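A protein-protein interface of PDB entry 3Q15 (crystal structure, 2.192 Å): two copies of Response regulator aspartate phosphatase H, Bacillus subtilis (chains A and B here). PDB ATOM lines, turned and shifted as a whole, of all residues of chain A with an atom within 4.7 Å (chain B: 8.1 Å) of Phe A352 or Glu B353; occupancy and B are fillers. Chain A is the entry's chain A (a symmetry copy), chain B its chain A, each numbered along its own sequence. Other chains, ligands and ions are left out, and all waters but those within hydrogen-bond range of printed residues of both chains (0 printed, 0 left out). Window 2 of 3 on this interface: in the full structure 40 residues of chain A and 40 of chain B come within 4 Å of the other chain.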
ATOM      1  N   GLU A 347     -30.611   1.480   4.636  1.00  0.00           N
ATOM      2  CA  GLU A 347     -30.027   1.600   3.304  1.00  0.00           C
ATOM      3  C   GLU A 347     -30.907   0.936   2.248  1.00  0.00           C
ATOM      4  O   GLU A 347     -31.037   1.441   1.134  1.00  0.00           O
ATOM      5  CB  GLU A 347     -28.630   0.981   3.255  1.00  0.00           C
ATOM      6  CG  GLU A 347     -27.508   1.901   3.694  1.00  0.00           C
ATOM      7  CD  GLU A 347     -26.142   1.293   3.437  1.00  0.00           C
ATOM      8  OE1 GLU A 347     -25.129   2.005   3.586  1.00  0.00           O
ATOM      9  OE2 GLU A 347     -26.086   0.097   3.078  1.00  0.00           O
ATOM     10  N   CYS A 350     -33.265   3.114   0.949  1.00  0.00           N
ATOM     11  CA  CYS A 350     -32.643   4.374   0.553  1.00  0.00           C
ATOM     12  C   CYS A 350     -32.815   5.482   1.594  1.00  0.00           C
ATOM     13  O   CYS A 350     -32.727   6.666   1.273  1.00  0.00           O
ATOM     14  CB  CYS A 350     -33.163   4.831  -0.816  1.00  0.00           C
ATOM     15  SG  CYS A 350     -32.668   3.757  -2.192  1.00  0.00           S
ATOM     16  N   HIS A 351     -33.060   5.090   2.840  1.00  0.00           N
ATOM     17  CA  HIS A 351     -33.104   6.043   3.943  1.00  0.00           C
ATOM     18  C   HIS A 351     -31.702   6.215   4.530  1.00  0.00           C
ATOM     19  O   HIS A 351     -31.374   5.651   5.577  1.00  0.00           O
ATOM     20  CB  HIS A 351     -34.101   5.587   5.006  1.00  0.00           C
ATOM     21  CG  HIS A 351     -35.529   5.784   4.608  1.00  0.00           C
ATOM     22  ND1 HIS A 351     -36.040   5.329   3.409  1.00  0.00           N
ATOM     23  CD2 HIS A 351     -36.556   6.400   5.240  1.00  0.00           C
ATOM     24  CE1 HIS A 351     -37.317   5.651   3.324  1.00  0.00           C
ATOM     25  NE2 HIS A 351     -37.656   6.302   4.423  1.00  0.00           N
ATOM     26  N   PHE A 352     -30.881   7.002   3.839  1.00  0.00           N
ATOM     27  CA  PHE A 352     -29.455   7.093   4.145  1.00  0.00           C
ATOM     28  C   PHE A 352     -29.131   7.970   5.352  1.00  0.00           C
ATOM     29  O   PHE A 352     -28.093   7.786   5.989  1.00  0.00           O
ATOM     30  CB  PHE A 352     -28.669   7.566   2.917  1.00  0.00           C
ATOM     31  CG  PHE A 352     -28.846   6.690   1.710  1.00  0.00           C
ATOM     32  CD1 PHE A 352     -28.273   5.431   1.663  1.00  0.00           C
ATOM     33  CD2 PHE A 352     -29.583   7.126   0.621  1.00  0.00           C
ATOM     34  CE1 PHE A 352     -28.429   4.621   0.561  1.00  0.00           C
ATOM     35  CE2 PHE A 352     -29.744   6.320  -0.490  1.00  0.00           C
ATOM     36  CZ  PHE A 352     -29.165   5.065  -0.518  1.00  0.00           C
ATOM     37  N   GLU A 353     -30.002   8.927   5.660  1.00  0.00           N
ATOM     38  CA  GLU A 353     -29.797   9.757   6.843  1.00  0.00           C
ATOM     39  C   GLU A 353     -29.869   8.882   8.087  1.00  0.00           C
ATOM     40  O   GLU A 353     -29.002   8.951   8.959  1.00  0.00           O
ATOM     41  CB  GLU A 353     -30.829  10.884   6.925  1.00  0.00           C
ATOM     42  CG  GLU A 353     -30.622  11.815   8.115  1.00  0.00           C
ATOM     43  CD  GLU A 353     -31.482  13.073   8.049  1.00  0.00           C
ATOM     44  OE1 GLU A 353     -32.348  13.178   7.149  1.00  0.00           O
ATOM     45  OE2 GLU A 353     -31.284  13.962   8.906  1.00  0.00           O
ATOM     46  N   GLN A 354     -30.909   8.059   8.161  1.00  0.00           N
ATOM     47  CA  GLN A 354     -31.041   7.091   9.239  1.00  0.00           C
ATOM     48  C   GLN A 354     -29.844   6.140   9.238  1.00  0.00           C
ATOM     49  O   GLN A 354     -29.281   5.834  10.286  1.00  0.00           O
ATOM     50  CB  GLN A 354     -32.347   6.303   9.105  1.00  0.00           C
ATOM     51  CG  GLN A 354     -33.609   7.124   9.355  1.00  0.00           C
ATOM     52  CD  GLN A 354     -34.196   7.725   8.085  1.00  0.00           C
ATOM     53  OE1 GLN A 354     -33.470   8.102   7.163  1.00  0.00           O
ATOM     54  NE2 GLN A 354     -35.520   7.812   8.032  1.00  0.00           N
ATOM     55  N   ALA A 355     -29.457   5.688   8.050  1.00  0.00           N
ATOM     56  CA  ALA A 355     -28.324   4.789   7.903  1.00  0.00           C
ATOM     57  C   ALA A 355     -27.060   5.403   8.493  1.00  0.00           C
ATOM     58  O   ALA A 355     -26.414   4.803   9.348  1.00  0.00           O
ATOM     59  CB  ALA A 355     -28.111   4.435   6.445  1.00  0.00           C
ATOM     60  N   ALA A 356     -26.712   6.599   8.032  1.00  0.00           N
ATOM     61  CA  ALA A 356     -25.523   7.291   8.517  1.00  0.00           C
ATOM     62  C   ALA A 356     -25.523   7.396  10.041  1.00  0.00           C
ATOM     63  O   ALA A 356     -24.493   7.194  10.686  1.00  0.00           O
ATOM     64  CB  ALA A 356     -25.414   8.672   7.883  1.00  0.00           C
ATOM     65  N   PHE B 346     -19.175  14.628   3.734  1.00  0.00           N
ATOM     66  CA  PHE B 346     -20.477  14.543   3.077  1.00  0.00           C
ATOM     67  C   PHE B 346     -21.639  14.714   4.056  1.00  0.00           C
ATOM     68  O   PHE B 346     -22.633  15.369   3.735  1.00  0.00           O
ATOM     69  CB  PHE B 346     -20.617  13.252   2.268  1.00  0.00           C
ATOM     70  CG  PHE B 346     -19.862  13.271   0.968  1.00  0.00           C
ATOM     71  CD1 PHE B 346     -20.301  14.045  -0.094  1.00  0.00           C
ATOM     72  CD2 PHE B 346     -18.714  12.511   0.806  1.00  0.00           C
ATOM     73  CE1 PHE B 346     -19.605  14.063  -1.291  1.00  0.00           C
ATOM     74  CE2 PHE B 346     -18.015  12.522  -0.388  1.00  0.00           C
ATOM     75  CZ  PHE B 346     -18.460  13.297  -1.437  1.00  0.00           C
ATOM     76  N   GLU B 347     -21.517  14.136   5.245  1.00  0.00           N
ATOM     77  CA  GLU B 347     -22.529  14.338   6.277  1.00  0.00           C
ATOM     78  C   GLU B 347     -22.738  15.821   6.569  1.00  0.00           C
ATOM     79  O   GLU B 347     -23.863  16.260   6.803  1.00  0.00           O
ATOM     80  CB  GLU B 347     -22.148  13.619   7.572  1.00  0.00           C
ATOM     81  CG  GLU B 347     -22.553  12.160   7.636  1.00  0.00           C
ATOM     82  CD  GLU B 347     -22.322  11.566   9.013  1.00  0.00           C
ATOM     83  OE1 GLU B 347     -22.769  10.429   9.261  1.00  0.00           O
ATOM     84  OE2 GLU B 347     -21.693  12.247   9.851  1.00  0.00           O
ATOM     85  N   CYS B 350     -25.150  17.232   4.524  1.00  0.00           N
ATOM     86  CA  CYS B 350     -26.359  16.413   4.509  1.00  0.00           C
ATOM     87  C   CYS B 350     -26.455  15.507   3.280  1.00  0.00           C
ATOM     88  O   CYS B 350     -27.542  15.075   2.901  1.00  0.00           O
ATOM     89  CB  CYS B 350     -27.612  17.289   4.636  1.00  0.00           C
ATOM     90  SG  CYS B 350     -27.778  18.116   6.243  1.00  0.00           S
ATOM     91  N   HIS B 351     -25.312  15.223   2.664  1.00  0.00           N
ATOM     92  CA  HIS B 351     -25.257  14.261   1.569  1.00  0.00           C
ATOM     93  C   HIS B 351     -25.021  12.858   2.129  1.00  0.00           C
ATOM     94  O   HIS B 351     -23.904  12.335   2.096  1.00  0.00           O
ATOM     95  CB  HIS B 351     -24.172  14.651   0.568  1.00  0.00           C
ATOM     96  CG  HIS B 351     -24.547  15.811  -0.298  1.00  0.00           C
ATOM     97  ND1 HIS B 351     -25.016  17.004   0.214  1.00  0.00           N
ATOM     98  CD2 HIS B 351     -24.537  15.961  -1.644  1.00  0.00           C
ATOM     99  CE1 HIS B 351     -25.275  17.836  -0.778  1.00  0.00           C
ATOM    100  NE2 HIS B 351     -24.993  17.228  -1.916  1.00  0.00           N
ATOM    101  N   PHE B 352     -26.091  12.258   2.646  1.00  0.00           N
ATOM    102  CA  PHE B 352     -25.989  11.018   3.412  1.00  0.00           C
ATOM    103  C   PHE B 352     -25.816   9.767   2.553  1.00  0.00           C
ATOM    104  O   PHE B 352     -25.277   8.764   3.021  1.00  0.00           O
ATOM    105  CB  PHE B 352     -27.193  10.859   4.346  1.00  0.00           C
ATOM    106  CG  PHE B 352     -27.370  12.002   5.305  1.00  0.00           C
ATOM    107  CD1 PHE B 352     -26.497  12.173   6.365  1.00  0.00           C
ATOM    108  CD2 PHE B 352     -28.411  12.903   5.148  1.00  0.00           C
ATOM    109  CE1 PHE B 352     -26.652  13.217   7.250  1.00  0.00           C
ATOM    110  CE2 PHE B 352     -28.574  13.952   6.032  1.00  0.00           C
ATOM    111  CZ  PHE B 352     -27.691  14.108   7.085  1.00  0.00           C
ATOM    112  N   GLU B 353     -26.283   9.816   1.307  1.00  0.00           N
ATOM    113  CA  GLU B 353     -26.088   8.686   0.403  1.00  0.00           C
ATOM    114  C   GLU B 353     -24.599   8.494   0.154  1.00  0.00           C
ATOM    115  O   GLU B 353     -24.080   7.382   0.254  1.00  0.00           O
ATOM    116  CB  GLU B 353     -26.828   8.891  -0.920  1.00  0.00           C
ATOM    117  CG  GLU B 353     -26.704   7.712  -1.878  1.00  0.00           C
ATOM    118  CD  GLU B 353     -27.645   7.808  -3.075  1.00  0.00           C
ATOM    119  OE1 GLU B 353     -28.311   8.856  -3.248  1.00  0.00           O
ATOM    120  OE2 GLU B 353     -27.717   6.824  -3.843  1.00  0.00           O
ATOM    121  N   GLN B 354     -23.918   9.587  -0.172  1.00  0.00           N
ATOM    122  CA  GLN B 354     -22.472   9.567  -0.328  1.00  0.00           C
ATOM    123  C   GLN B 354     -21.810   9.119   0.975  1.00  0.00           C
ATOM    124  O   GLN B 354     -20.888   8.308   0.968  1.00  0.00           O
ATOM    125  CB  GLN B 354     -21.950  10.945  -0.745  1.00  0.00           C
ATOM    126  CG  GLN B 354     -22.345  11.370  -2.156  1.00  0.00           C
ATOM    127  CD  GLN B 354     -23.634  12.180  -2.201  1.00  0.00           C
ATOM    128  OE1 GLN B 354     -24.558  11.952  -1.418  1.00  0.00           O
ATOM    129  NE2 GLN B 354     -23.696  13.137  -3.121  1.00  0.00           N
ATOM    130  N   ALA B 355     -22.300   9.649   2.091  1.00  0.00           N
ATOM    131  CA  ALA B 355     -21.774   9.300   3.401  1.00  0.00           C
ATOM    132  C   ALA B 355     -21.857   7.797   3.639  1.00  0.00           C
ATOM    133  O   ALA B 355     -20.853   7.156   3.941  1.00  0.00           O
ATOM    134  CB  ALA B 355     -22.516  10.051   4.489  1.00  0.00           C
ATOM    135  N   ALA B 356     -23.055   7.241   3.504  1.00  0.00           N
ATOM    136  CA  ALA B 356     -23.264   5.811   3.706  1.00  0.00           C
ATOM    137  C   ALA B 356     -22.302   4.983   2.856  1.00  0.00           C
ATOM    138  O   ALA B 356     -21.744   3.990   3.325  1.00  0.00           O
ATOM    139  CB  ALA B 356     -24.709   5.435   3.404  1.00  0.00           C
ATOM    140  N   ALA B 357     -22.109   5.397   1.607  1.00  0.00           N
ATOM    141  CA  ALA B 357     -21.180   4.707   0.716  1.00  0.00           C
ATOM    142  C   ALA B 357     -19.774   4.621   1.315  1.00  0.00           C
ATOM    143  O   ALA B 357     -19.127   3.575   1.258  1.00  0.00           O
ATOM    144  CB  ALA B 357     -21.140   5.387  -0.647  1.00  0.00           C
ATOM    145  N   PHE B 358     -19.306   5.724   1.890  1.00  0.00           N
ATOM    146  CA  PHE B 358     -17.976   5.746   2.483  1.00  0.00           C
ATOM    147  C   PHE B 358     -17.918   4.973   3.791  1.00  0.00           C
ATOM    148  O   PHE B 358     -16.912   4.341   4.089  1.00  0.00           O
ATOM    149  CB  PHE B 358     -17.466   7.179   2.647  1.00  0.00           C
ATOM    150  CG  PHE B 358     -17.021   7.800   1.357  1.00  0.00           C
ATOM    151  CD1 PHE B 358     -17.839   8.679   0.678  1.00  0.00           C
ATOM    152  CD2 PHE B 358     -15.793   7.472   0.807  1.00  0.00           C
ATOM    153  CE1 PHE B 358     -17.435   9.236  -0.517  1.00  0.00           C
ATOM    154  CE2 PHE B 358     -15.383   8.026  -0.388  1.00  0.00           C
ATOM    155  CZ  PHE B 358     -16.206   8.908  -1.051  1.00  0.00           C
ATOM    156  N   TYR B 359     -19.002   5.007   4.559  1.00  0.00           N
ATOM    157  CA  TYR B 359     -19.080   4.215   5.781  1.00  0.00           C
ATOM    158  C   TYR B 359     -18.932   2.724   5.467  1.00  0.00           C
ATOM    159  O   TYR B 359     -18.300   1.984   6.219  1.00  0.00           O
ATOM    160  CB  TYR B 359     -20.399   4.474   6.516  1.00  0.00           C
ATOM    161  CG  TYR B 359     -20.427   5.745   7.342  1.00  0.00           C
ATOM    162  CD1 TYR B 359     -19.345   6.103   8.131  1.00  0.00           C
ATOM    163  CD2 TYR B 359     -21.536   6.583   7.330  1.00  0.00           C
ATOM    164  CE1 TYR B 359     -19.363   7.254   8.887  1.00  0.00           C
ATOM    165  CE2 TYR B 359     -21.562   7.744   8.086  1.00  0.00           C
ATOM    166  CZ  TYR B 359     -20.473   8.072   8.860  1.00  0.00           C
ATOM    167  OH  TYR B 359     -20.488   9.223   9.616  1.00  0.00           O
ATOM    168  N   ARG B 360     -19.512   2.286   4.353  1.00  0.00           N
ATOM    169  CA  ARG B 360     -19.380   0.893   3.934  1.00  0.00           C
ATOM    170  C   ARG B 360     -17.937   0.562   3.549  1.00  0.00           C
ATOM    171  O   ARG B 360     -17.457  -0.545   3.796  1.00  0.00           O
ATOM    172  CB  ARG B 360     -20.331   0.566   2.776  1.00  0.00           C
ATOM    173  CG  ARG B 360     -21.811   0.568   3.147  1.00  0.00           C
ATOM    174  CD  ARG B 360     -22.688  -0.109   2.073  1.00  0.00           C
ATOM    175  NE  ARG B 360     -22.539   0.496   0.751  1.00  0.00           N
ATOM    176  CZ  ARG B 360     -23.196   1.579   0.342  1.00  0.00           C
ATOM    177  NH1 ARG B 360     -24.053   2.180   1.154  1.00  0.00           N
ATOM    178  NH2 ARG B 360     -22.996   2.066  -0.878  1.00  0.00           N
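The side-chain carboxylate of Glu B347 sits at hydrogen-bond distance from the side-chain hydroxyl of Tyr B359 (2.6 Å).
Glu A347 touches Ala B356, and with the chains exchanged Ala A356 touches Glu B347.
Phe A352 touches its own counterpart, Phe B352.
Phe A352 touches Glu B353, and with the chains exchanged Glu A353 touches Phe B352.
Phe A352 touches Ala B356, and with the chains exchanged Ala A356 touches Phe B352.
8 positions are printed for both chains.
Of the 9 pairs that touch across the chains among the printed residues, 7 have their exchanged pair printed and touching as well.
Among the printed residues, pairs that only touch across the chains: Glu A347 with Ala B356 (3.5 Å), Phe A352 with Phe B352 (3.6 Å), Phe A352 with Glu B353 (3.6 Å), Phe A352 with Ala B356 (3.97 Å), Glu A353 with Phe B352 (3.6 Å), Ala A356 with Glu B347 (3.5 Å), Ala A356 with Phe B352 (3.97 Å) and Ala A356 with Tyr B359 (3.96 Å).
NH1 of Arg B360 lies within salt-bridge range of OE1 of Glu A347, 2.7 Å away.
Printed residues of chain B that touch a printed residue of chain A: Glu B347, Phe B352, Glu B353, Ala B356, Tyr B359 and Arg B360.
Hydrophobic or aromatic side chains of chain B within 4 Å of the printed part of chain A: Phe B352, Ala B356 and Tyr B359.
Hydrophobic or aromatic side chains of chain A that line the printed part of chain B: Phe A352 and Ala A356.
Among the printed residues, Asp or Glu carboxylates within 4 Å of a Lys or Arg side-chain nitrogen of the other chain: Glu A347 with Arg B360.
Phe A352 touches just these residues of chain B: Phe B352 (3.6 Å), Glu B353 (3.6 Å) and Ala B356 (3.97 Å).
Of chain A, only Phe A352 (3.6 Å) comes within 4 Å of Glu B353.
Printed residues of chain A within 4 Å of Phe B352: Phe A352 (3.6 Å), Glu A353 (3.6 Å) and Ala A356 (3.97 Å).
Printed residues of chain B within 4 Å of Glu A353: Phe B352 (3.6 Å).
Of the printed residues of chain B, Ala A356 touches Glu B347, Phe B352 and Tyr B359.
Of the printed residues of chain A, Ala B356 touches Glu A347 (3.5 Å) and Phe A352 (3.97 Å).
Gln B354 touches none of the printed residues of chain A.
The nearest residue of chain B that does not touch Phe A352 is Arg B360 (5.0 Å).
The nearest printed residue of chain B that does not touch Glu A353 is Glu B353 (5.8 Å).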
